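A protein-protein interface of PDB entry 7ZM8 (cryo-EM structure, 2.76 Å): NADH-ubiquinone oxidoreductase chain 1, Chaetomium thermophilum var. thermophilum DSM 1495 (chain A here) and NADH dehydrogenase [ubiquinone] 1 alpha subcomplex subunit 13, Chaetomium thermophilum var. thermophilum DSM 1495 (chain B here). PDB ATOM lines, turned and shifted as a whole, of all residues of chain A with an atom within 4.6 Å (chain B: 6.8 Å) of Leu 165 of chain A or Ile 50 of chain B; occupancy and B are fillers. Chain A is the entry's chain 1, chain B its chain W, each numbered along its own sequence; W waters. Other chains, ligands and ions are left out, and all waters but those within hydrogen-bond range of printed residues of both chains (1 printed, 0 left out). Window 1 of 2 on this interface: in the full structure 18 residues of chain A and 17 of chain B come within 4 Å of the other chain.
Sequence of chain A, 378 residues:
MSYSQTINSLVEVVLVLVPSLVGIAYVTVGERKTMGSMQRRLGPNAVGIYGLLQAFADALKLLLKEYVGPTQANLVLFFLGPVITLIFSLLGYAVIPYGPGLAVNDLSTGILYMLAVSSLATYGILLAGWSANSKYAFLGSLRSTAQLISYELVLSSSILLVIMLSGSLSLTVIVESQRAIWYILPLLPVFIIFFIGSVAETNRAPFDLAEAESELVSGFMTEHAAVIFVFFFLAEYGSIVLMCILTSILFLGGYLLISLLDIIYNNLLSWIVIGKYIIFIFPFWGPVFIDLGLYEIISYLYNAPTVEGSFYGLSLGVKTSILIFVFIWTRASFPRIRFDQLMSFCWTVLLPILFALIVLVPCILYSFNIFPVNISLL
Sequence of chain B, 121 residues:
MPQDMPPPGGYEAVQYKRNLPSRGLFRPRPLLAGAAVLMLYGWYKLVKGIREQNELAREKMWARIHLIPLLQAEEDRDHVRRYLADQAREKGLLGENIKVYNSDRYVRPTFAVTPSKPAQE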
ATOM      1  N   LEU A 161      -1.186  24.047  32.724  1.00  0.00           N
ATOM      2  CA  LEU A 161      -2.500  24.557  32.360  1.00  0.00           C
ATOM      3  C   LEU A 161      -2.642  24.744  30.856  1.00  0.00           C
ATOM      4  O   LEU A 161      -3.756  24.694  30.330  1.00  0.00           O
ATOM      5  CB  LEU A 161      -2.763  25.868  33.098  1.00  0.00           C
ATOM      6  CG  LEU A 161      -3.008  25.703  34.595  1.00  0.00           C
ATOM      7  CD1 LEU A 161      -2.581  26.937  35.357  1.00  0.00           C
ATOM      8  CD2 LEU A 161      -4.466  25.381  34.859  1.00  0.00           C
ATOM      9  N   VAL A 162      -1.535  24.984  30.155  1.00  0.00           N
ATOM     10  CA  VAL A 162      -1.567  25.014  28.695  1.00  0.00           C
ATOM     11  C   VAL A 162      -1.745  23.609  28.137  1.00  0.00           C
ATOM     12  O   VAL A 162      -2.491  23.398  27.177  1.00  0.00           O
ATOM     13  CB  VAL A 162      -0.292  25.687  28.149  1.00  0.00           C
ATOM     14  CG1 VAL A 162      -0.174  25.483  26.654  1.00  0.00           C
ATOM     15  CG2 VAL A 162      -0.281  27.169  28.494  1.00  0.00           C
ATOM     16  N   ILE A 163      -1.067  22.627  28.734  1.00  0.00           N
ATOM     17  CA  ILE A 163      -1.141  21.250  28.261  1.00  0.00           C
ATOM     18  C   ILE A 163      -2.556  20.712  28.376  1.00  0.00           C
ATOM     19  O   ILE A 163      -2.984  19.891  27.558  1.00  0.00           O
ATOM     20  CB  ILE A 163      -0.135  20.378  29.037  1.00  0.00           C
ATOM     21  CG1 ILE A 163       1.254  21.029  29.035  1.00  0.00           C
ATOM     22  CG2 ILE A 163      -0.075  18.975  28.455  1.00  0.00           C
ATOM     23  CD1 ILE A 163       1.874  21.180  27.666  1.00  0.00           C
ATOM     24  N   MET A 164      -3.283  21.145  29.405  1.00  0.00           N
ATOM     25  CA  MET A 164      -4.705  20.772  29.573  1.00  0.00           C
ATOM     26  C   MET A 164      -5.537  21.262  28.386  1.00  0.00           C
ATOM     27  O   MET A 164      -6.356  20.482  27.919  1.00  0.00           O
ATOM     28  CB  MET A 164      -5.216  21.361  30.881  1.00  0.00           C
ATOM     29  CG  MET A 164      -4.750  20.585  32.091  1.00  0.00           C
ATOM     30  SD  MET A 164      -5.230  21.358  33.643  1.00  0.00           S
ATOM     31  CE  MET A 164      -4.486  20.231  34.818  1.00  0.00           C
ATOM     32  N   LEU A 165      -5.358  22.500  27.930  1.00  0.00           N
ATOM     33  CA  LEU A 165      -6.083  23.035  26.744  1.00  0.00           C
ATOM     34  C   LEU A 165      -5.601  22.424  25.428  1.00  0.00           C
ATOM     35  O   LEU A 165      -6.438  22.190  24.559  1.00  0.00           O
ATOM     36  CB  LEU A 165      -5.981  24.563  26.698  1.00  0.00           C
ATOM     37  CG  LEU A 165      -6.272  25.333  27.979  1.00  0.00           C
ATOM     38  CD1 LEU A 165      -6.392  26.805  27.651  1.00  0.00           C
ATOM     39  CD2 LEU A 165      -7.547  24.843  28.642  1.00  0.00           C
ATOM     40  N   SER A 166      -4.300  22.221  25.280  1.00  0.00           N
ATOM     41  CA  SER A 166      -3.699  21.723  24.019  1.00  0.00           C
ATOM     42  C   SER A 166      -3.870  20.215  23.896  1.00  0.00           C
ATOM     43  O   SER A 166      -4.218  19.756  22.807  1.00  0.00           O
ATOM     44  CB  SER A 166      -2.249  22.126  23.933  1.00  0.00           C
ATOM     45  OG  SER A 166      -1.644  21.584  22.774  1.00  0.00           O
ATOM     46  N   GLY A 167      -3.639  19.492  24.981  1.00  0.00           N
ATOM     47  CA  GLY A 167      -3.662  18.051  24.934  1.00  0.00           C
ATOM     48  C   GLY A 167      -2.334  17.397  24.625  1.00  0.00           C
ATOM     49  O   GLY A 167      -2.221  16.175  24.754  1.00  0.00           O
ATOM     50  N   TYR A 183      -3.573  31.571  23.640  1.00  0.00           N
ATOM     51  CA  TYR A 183      -3.811  31.128  25.040  1.00  0.00           C
ATOM     52  C   TYR A 183      -3.753  32.280  26.038  1.00  0.00           C
ATOM     53  O   TYR A 183      -4.191  32.080  27.159  1.00  0.00           O
ATOM     54  CB  TYR A 183      -2.944  29.910  25.362  1.00  0.00           C
ATOM     55  CG  TYR A 183      -3.440  28.633  24.740  1.00  0.00           C
ATOM     56  CD1 TYR A 183      -4.673  28.587  24.115  1.00  0.00           C
ATOM     57  CD2 TYR A 183      -2.679  27.478  24.765  1.00  0.00           C
ATOM     58  CE1 TYR A 183      -5.139  27.423  23.529  1.00  0.00           C
ATOM     59  CE2 TYR A 183      -3.131  26.304  24.188  1.00  0.00           C
ATOM     60  CZ  TYR A 183      -4.366  26.280  23.570  1.00  0.00           C
ATOM     61  OH  TYR A 183      -4.823  25.132  23.006  1.00  0.00           O
ATOM     62  N   LEU A 187      -6.431  32.216  29.122  1.00  0.00           N
ATOM     63  CA  LEU A 187      -5.606  31.944  30.291  1.00  0.00           C
ATOM     64  C   LEU A 187      -4.858  33.198  30.706  1.00  0.00           C
ATOM     65  O   LEU A 187      -3.648  33.151  30.931  1.00  0.00           O
ATOM     66  CB  LEU A 187      -4.610  30.819  30.025  1.00  0.00           C
ATOM     67  CG  LEU A 187      -5.113  29.417  29.712  1.00  0.00           C
ATOM     68  CD1 LEU A 187      -3.934  28.507  29.443  1.00  0.00           C
ATOM     69  CD2 LEU A 187      -5.960  28.868  30.839  1.00  0.00           C
ATOM     70  N   VAL A 361      -9.618  24.640  35.916  1.00  0.00           N
ATOM     71  CA  VAL A 361      -9.563  24.556  34.455  1.00  0.00           C
ATOM     72  C   VAL A 361     -10.043  23.211  33.921  1.00  0.00           C
ATOM     73  O   VAL A 361     -10.862  23.201  32.990  1.00  0.00           O
ATOM     74  CB  VAL A 361      -8.155  24.933  33.958  1.00  0.00           C
ATOM     75  CG1 VAL A 361      -7.940  24.455  32.543  1.00  0.00           C
ATOM     76  CG2 VAL A 361      -7.972  26.431  34.035  1.00  0.00           C
ATOM     77  N   LEU A 365     -13.315  22.469  31.538  1.00  0.00           N
ATOM     78  CA  LEU A 365     -13.126  21.746  30.285  1.00  0.00           C
ATOM     79  C   LEU A 365     -14.097  20.580  30.174  1.00  0.00           C
ATOM     80  O   LEU A 365     -14.678  20.348  29.111  1.00  0.00           O
ATOM     81  CB  LEU A 365     -11.686  21.254  30.171  1.00  0.00           C
ATOM     82  CG  LEU A 365     -10.602  22.252  29.781  1.00  0.00           C
ATOM     83  CD1 LEU A 365      -9.290  21.546  29.483  1.00  0.00           C
ATOM     84  CD2 LEU A 365     -11.036  23.062  28.595  1.00  0.00           C
ATOM     85  N   ILE A 370     -14.993  19.923  26.425  1.00  0.00           N
ATOM     86  CA  ILE A 370     -13.885  20.545  25.644  1.00  0.00           C
ATOM     87  C   ILE A 370     -12.543  19.904  25.915  1.00  0.00           C
ATOM     88  O   ILE A 370     -11.547  20.560  25.633  1.00  0.00           O
ATOM     89  CB  ILE A 370     -13.879  22.088  25.633  1.00  0.00           C
ATOM     90  CG1 ILE A 370     -14.207  22.712  26.986  1.00  0.00           C
ATOM     91  CG2 ILE A 370     -14.803  22.607  24.545  1.00  0.00           C
ATOM     92  CD1 ILE A 370     -13.942  24.192  27.035  1.00  0.00           C
ATOM     93  N   PHE A 371     -12.515  18.747  26.567  1.00  0.00           N
ATOM     94  CA  PHE A 371     -11.274  17.986  26.558  1.00  0.00           C
ATOM     95  C   PHE A 371     -10.850  17.735  25.116  1.00  0.00           C
ATOM     96  O   PHE A 371     -11.655  17.245  24.317  1.00  0.00           O
ATOM     97  CB  PHE A 371     -11.428  16.654  27.294  1.00  0.00           C
ATOM     98  CG  PHE A 371     -11.489  16.771  28.787  1.00  0.00           C
ATOM     99  CD1 PHE A 371     -11.035  17.899  29.429  1.00  0.00           C
ATOM    100  CD2 PHE A 371     -12.024  15.755  29.546  1.00  0.00           C
ATOM    101  CE1 PHE A 371     -11.080  17.993  30.796  1.00  0.00           C
ATOM    102  CE2 PHE A 371     -12.083  15.858  30.913  1.00  0.00           C
ATOM    103  CZ  PHE A 371     -11.611  16.979  31.536  1.00  0.00           C
ATOM    104  N   PRO A 372      -9.625  18.078  24.736  1.00  0.00           N
ATOM    105  CA  PRO A 372      -9.148  17.734  23.399  1.00  0.00           C
ATOM    106  C   PRO A 372      -8.748  16.270  23.320  1.00  0.00           C
ATOM    107  O   PRO A 372      -8.613  15.576  24.324  1.00  0.00           O
ATOM    108  CB  PRO A 372      -7.935  18.650  23.213  1.00  0.00           C
ATOM    109  CG  PRO A 372      -7.451  18.891  24.575  1.00  0.00           C
ATOM    110  CD  PRO A 372      -8.641  18.878  25.484  1.00  0.00           C
ATOM    111  N   TRP B  43     -12.464  32.349  26.117  1.00  0.00           N
ATOM    112  CA  TRP B  43     -13.085  31.096  26.528  1.00  0.00           C
ATOM    113  C   TRP B  43     -14.221  30.708  25.598  1.00  0.00           C
ATOM    114  O   TRP B  43     -14.477  29.518  25.401  1.00  0.00           O
ATOM    115  CB  TRP B  43     -13.566  31.197  27.969  1.00  0.00           C
ATOM    116  CG  TRP B  43     -12.531  30.750  28.919  1.00  0.00           C
ATOM    117  CD1 TRP B  43     -11.817  31.523  29.775  1.00  0.00           C
ATOM    118  CD2 TRP B  43     -12.067  29.414  29.101  1.00  0.00           C
ATOM    119  NE1 TRP B  43     -10.940  30.753  30.491  1.00  0.00           N
ATOM    120  CE2 TRP B  43     -11.073  29.451  30.092  1.00  0.00           C
ATOM    121  CE3 TRP B  43     -12.402  28.187  28.524  1.00  0.00           C
ATOM    122  CZ2 TRP B  43     -10.405  28.312  30.517  1.00  0.00           C
ATOM    123  CZ3 TRP B  43     -11.741  27.063  28.947  1.00  0.00           C
ATOM    124  CH2 TRP B  43     -10.753  27.129  29.935  1.00  0.00           C
ATOM    125  N   LYS B  45     -13.959  31.291  22.294  1.00  0.00           N
ATOM    126  CA  LYS B  45     -13.220  30.853  21.086  1.00  0.00           C
ATOM    127  C   LYS B  45     -12.508  29.518  21.342  1.00  0.00           C
ATOM    128  O   LYS B  45     -12.309  28.784  20.376  1.00  0.00           O
ATOM    129  CB  LYS B  45     -12.343  32.025  20.634  1.00  0.00           C
ATOM    130  CG  LYS B  45     -13.093  33.292  20.267  1.00  0.00           C
ATOM    131  CD  LYS B  45     -13.792  33.202  18.938  1.00  0.00           C
ATOM    132  CE  LYS B  45     -12.833  33.163  17.770  1.00  0.00           C
ATOM    133  NZ  LYS B  45     -13.541  32.931  16.491  1.00  0.00           N
ATOM    134  N   LEU B  46     -12.091  29.244  22.579  1.00  0.00           N
ATOM    135  CA  LEU B  46     -11.502  27.938  22.963  1.00  0.00           C
ATOM    136  C   LEU B  46     -12.582  26.868  22.908  1.00  0.00           C
ATOM    137  O   LEU B  46     -12.274  25.756  22.494  1.00  0.00           O
ATOM    138  CB  LEU B  46     -10.935  28.027  24.378  1.00  0.00           C
ATOM    139  CG  LEU B  46      -9.997  26.891  24.770  1.00  0.00           C
ATOM    140  CD1 LEU B  46      -8.772  26.860  23.873  1.00  0.00           C
ATOM    141  CD2 LEU B  46      -9.589  27.024  26.219  1.00  0.00           C
ATOM    142  N   VAL B  47     -13.804  27.208  23.287  1.00  0.00           N
ATOM    143  CA  VAL B  47     -14.878  26.188  23.347  1.00  0.00           C
ATOM    144  C   VAL B  47     -15.144  25.736  21.925  1.00  0.00           C
ATOM    145  O   VAL B  47     -15.118  24.534  21.666  1.00  0.00           O
ATOM    146  CB  VAL B  47     -16.151  26.630  24.102  1.00  0.00           C
ATOM    147  CG1 VAL B  47     -17.350  25.760  23.763  1.00  0.00           C
ATOM    148  CG2 VAL B  47     -15.944  26.686  25.606  1.00  0.00           C
ATOM    149  N   LYS B  48     -15.316  26.689  21.030  1.00  0.00           N
ATOM    150  CA  LYS B  48     -15.616  26.338  19.624  1.00  0.00           C
ATOM    151  C   LYS B  48     -14.451  25.601  18.960  1.00  0.00           C
ATOM    152  O   LYS B  48     -14.720  24.641  18.234  1.00  0.00           O
ATOM    153  CB  LYS B  48     -15.870  27.625  18.842  1.00  0.00           C
ATOM    154  CG  LYS B  48     -17.034  28.489  19.282  1.00  0.00           C
ATOM    155  CD  LYS B  48     -17.296  29.574  18.274  1.00  0.00           C
ATOM    156  CE  LYS B  48     -17.315  29.054  16.853  1.00  0.00           C
ATOM    157  NZ  LYS B  48     -17.574  30.137  15.875  1.00  0.00           N
ATOM    158  N   GLY B  49     -13.219  26.050  19.169  1.00  0.00           N
ATOM    159  CA  GLY B  49     -12.075  25.427  18.494  1.00  0.00           C
ATOM    160  C   GLY B  49     -11.883  23.984  18.891  1.00  0.00           C
ATOM    161  O   GLY B  49     -11.656  23.162  18.009  1.00  0.00           O
ATOM    162  N   ILE B  50     -11.897  23.687  20.188  1.00  0.00           N
ATOM    163  CA  ILE B  50     -11.603  22.290  20.613  1.00  0.00           C
ATOM    164  C   ILE B  50     -12.727  21.394  20.093  1.00  0.00           C
ATOM    165  O   ILE B  50     -12.454  20.237  19.762  1.00  0.00           O
ATOM    166  CB  ILE B  50     -11.396  22.198  22.137  1.00  0.00           C
ATOM    167  CG1 ILE B  50     -10.317  23.170  22.613  1.00  0.00           C
ATOM    168  CG2 ILE B  50     -11.076  20.773  22.545  1.00  0.00           C
ATOM    169  CD1 ILE B  50     -10.046  23.113  24.095  1.00  0.00           C
ATOM    170  N   ARG B  51     -13.943  21.925  20.005  1.00  0.00           N
ATOM    171  CA  ARG B  51     -15.088  21.152  19.459  1.00  0.00           C
ATOM    172  C   ARG B  51     -14.828  20.824  17.982  1.00  0.00           C
ATOM    173  O   ARG B  51     -15.168  19.711  17.566  1.00  0.00           O
ATOM    174  CB  ARG B  51     -16.393  21.877  19.791  1.00  0.00           C
ATOM    175  CG  ARG B  51     -16.897  21.603  21.198  1.00  0.00           C
ATOM    176  CD  ARG B  51     -18.189  22.327  21.516  1.00  0.00           C
ATOM    177  NE  ARG B  51     -18.699  21.962  22.829  1.00  0.00           N
ATOM    178  CZ  ARG B  51     -19.742  22.540  23.410  1.00  0.00           C
ATOM    179  NH1 ARG B  51     -20.139  22.142  24.605  1.00  0.00           N
ATOM    180  NH2 ARG B  51     -20.382  23.517  22.796  1.00  0.00           N
ATOM    181  N   GLU B  52     -14.231  21.751  17.228  1.00  0.00           N
ATOM    182  CA  GLU B  52     -13.871  21.503  15.806  1.00  0.00           C
ATOM    183  C   GLU B  52     -12.723  20.491  15.730  1.00  0.00           C
ATOM    184  O   GLU B  52     -12.792  19.609  14.864  1.00  0.00           O
ATOM    185  CB  GLU B  52     -13.513  22.824  15.127  1.00  0.00           C
ATOM    186  CG  GLU B  52     -13.130  22.696  13.667  1.00  0.00           C
ATOM    187  CD  GLU B  52     -13.554  23.879  12.810  1.00  0.00           C
ATOM    188  OE1 GLU B  52     -14.545  24.546  13.171  1.00  0.00           O
ATOM    189  OE2 GLU B  52     -12.893  24.129  11.786  1.00  0.00           O
ATOM    190  N   GLN B  53     -11.719  20.605  16.599  1.00  0.00           N
ATOM    191  CA  GLN B  53     -10.562  19.685  16.606  1.00  0.00           C
ATOM    192  C   GLN B  53     -11.063  18.274  16.855  1.00  0.00           C
ATOM    193  O   GLN B  53     -10.515  17.348  16.273  1.00  0.00           O
ATOM    194  CB  GLN B  53      -9.633  20.002  17.770  1.00  0.00           C
ATOM    195  CG  GLN B  53      -8.334  20.683  17.388  1.00  0.00           C
ATOM    196  CD  GLN B  53      -7.590  21.066  18.640  1.00  0.00           C
ATOM    197  OE1 GLN B  53      -7.950  20.658  19.739  1.00  0.00           O
ATOM    198  NE2 GLN B  53      -6.544  21.856  18.486  1.00  0.00           N
ATOM    199  N   ASN B  54     -12.060  18.123  17.712  1.00  0.00           N
ATOM    200  CA  ASN B  54     -12.533  16.781  18.117  1.00  0.00           C
ATOM    201  C   ASN B  54     -13.360  16.166  16.999  1.00  0.00           C
ATOM    202  O   ASN B  54     -13.477  14.946  16.974  1.00  0.00           O
ATOM    203  CB  ASN B  54     -13.240  16.860  19.464  1.00  0.00           C
ATOM    204  CG  ASN B  54     -12.312  17.053  20.640  1.00  0.00           C
ATOM    205  OD1 ASN B  54     -11.101  17.139  20.480  1.00  0.00           O
ATOM    206  ND2 ASN B  54     -12.872  17.122  21.834  1.00  0.00           N
ATOM    207  N   GLU B  55     -13.891  16.995  16.112  1.00  0.00           N
ATOM    208  CA  GLU B  55     -14.671  16.507  14.953  1.00  0.00           C
ATOM    209  C   GLU B  55     -13.724  16.264  13.774  1.00  0.00           C
ATOM    210  O   GLU B  55     -14.030  15.424  12.929  1.00  0.00           O
ATOM    211  CB  GLU B  55     -15.837  17.472  14.729  1.00  0.00           C
ATOM    212  CG  GLU B  55     -16.880  17.401  15.823  1.00  0.00           C
ATOM    213  CD  GLU B  55     -17.254  15.989  16.238  1.00  0.00           C
ATOM    214  OE1 GLU B  55     -17.320  15.731  17.457  1.00  0.00           O
ATOM    215  OE2 GLU B  55     -17.497  15.154  15.342  1.00  0.00           O
HETATM  216  O   HOH W   1     -14.350  15.904  24.729  1.00  0.00           O
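Water W1 lies within hydrogen-bond range of O of Phe 371 of chain A (3.0 Å) and ND2 of Asn 54 of chain B (3.5 Å).
Leu 165 of chain A touches two residues of chain B. Printed residues of chain B within 4 Å of Tyr 183 of chain A: Leu 46 (3.7 Å). Printed residues of chain B within 4 Å of Ile 370 of chain A: Val 47 (3.5 Å) and Ile 50 (3.1 Å). Of the printed residues of chain B, Pro 372 of chain A touches Ile 50 (3.7 Å) and Asn 54 (3.6 Å). Printed residues of chain A within 4 Å of Leu 46 of chain B: Leu 165 (3.5 Å) and Tyr 183 (3.7 Å). Of the printed residues of chain A, Val 47 of chain B touches Ile 370. Printed residues of chain A within 4 Å of Ile 50 of chain B: Leu 165 (3.8 Å), Ile 370 (3.1 Å), Phe 371 (3.99 Å) and Pro 372 (3.7 Å). The nearest printed residue of chain B that does not touch Pro 372 of chain A is Gln 53 of chain B (4.01 Å).
The side-chain amide nitrogen (ND2) of Asn 54 of chain B lies within hydrogen-bond range of the backbone carbonyl oxygen (O) of Phe 371 of chain A (2.8 Å).
Hydrophobic or aromatic side chains of chain B that line the printed part of chain A: Leu 46, Val 47 and Ile 50. Hydrophobic or aromatic side chains of chain A within 4 Å of the printed part of chain B: Leu 165, Tyr 183, Ile 370 and Pro 372. Along chain A the printed residues that touch a printed residue of chain B span positions 165 to 372. Among the printed residues, no Asp or Glu carboxylate lies within 4 Å of a Lys or Arg side-chain nitrogen of the other chain.
CD1 of Leu 165 of chain A touches CD2 of Leu 46 of chain B, at 3.5 Å. O of Leu 165 of chain A touches CD1 of Ile 50 of chain B, at 3.8 Å. Tyr 183 of chain A touches Leu 46 of chain B (CE1 to CD1, 3.7 Å). Ile 370 of chain A touches Val 47 of chain B. CG2 of Ile 50 of chain B touches O of Ile 370 of chain A (3.1 Å). Phe 371 of chain A touches Ile 50 of chain B. Ile 50 of chain B touches Pro 372 of chain A. Asn 54 of chain B touches Pro 372 of chain A.
O of Leu 365 of chain A sits at hydrogen-bond distance from N of Ile 370 of chain A (2.7 Å). The side-chain amide oxygen of Asn 54 of chain B lies close to the backbone carbonyl oxygen of Ile 50 of chain B.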
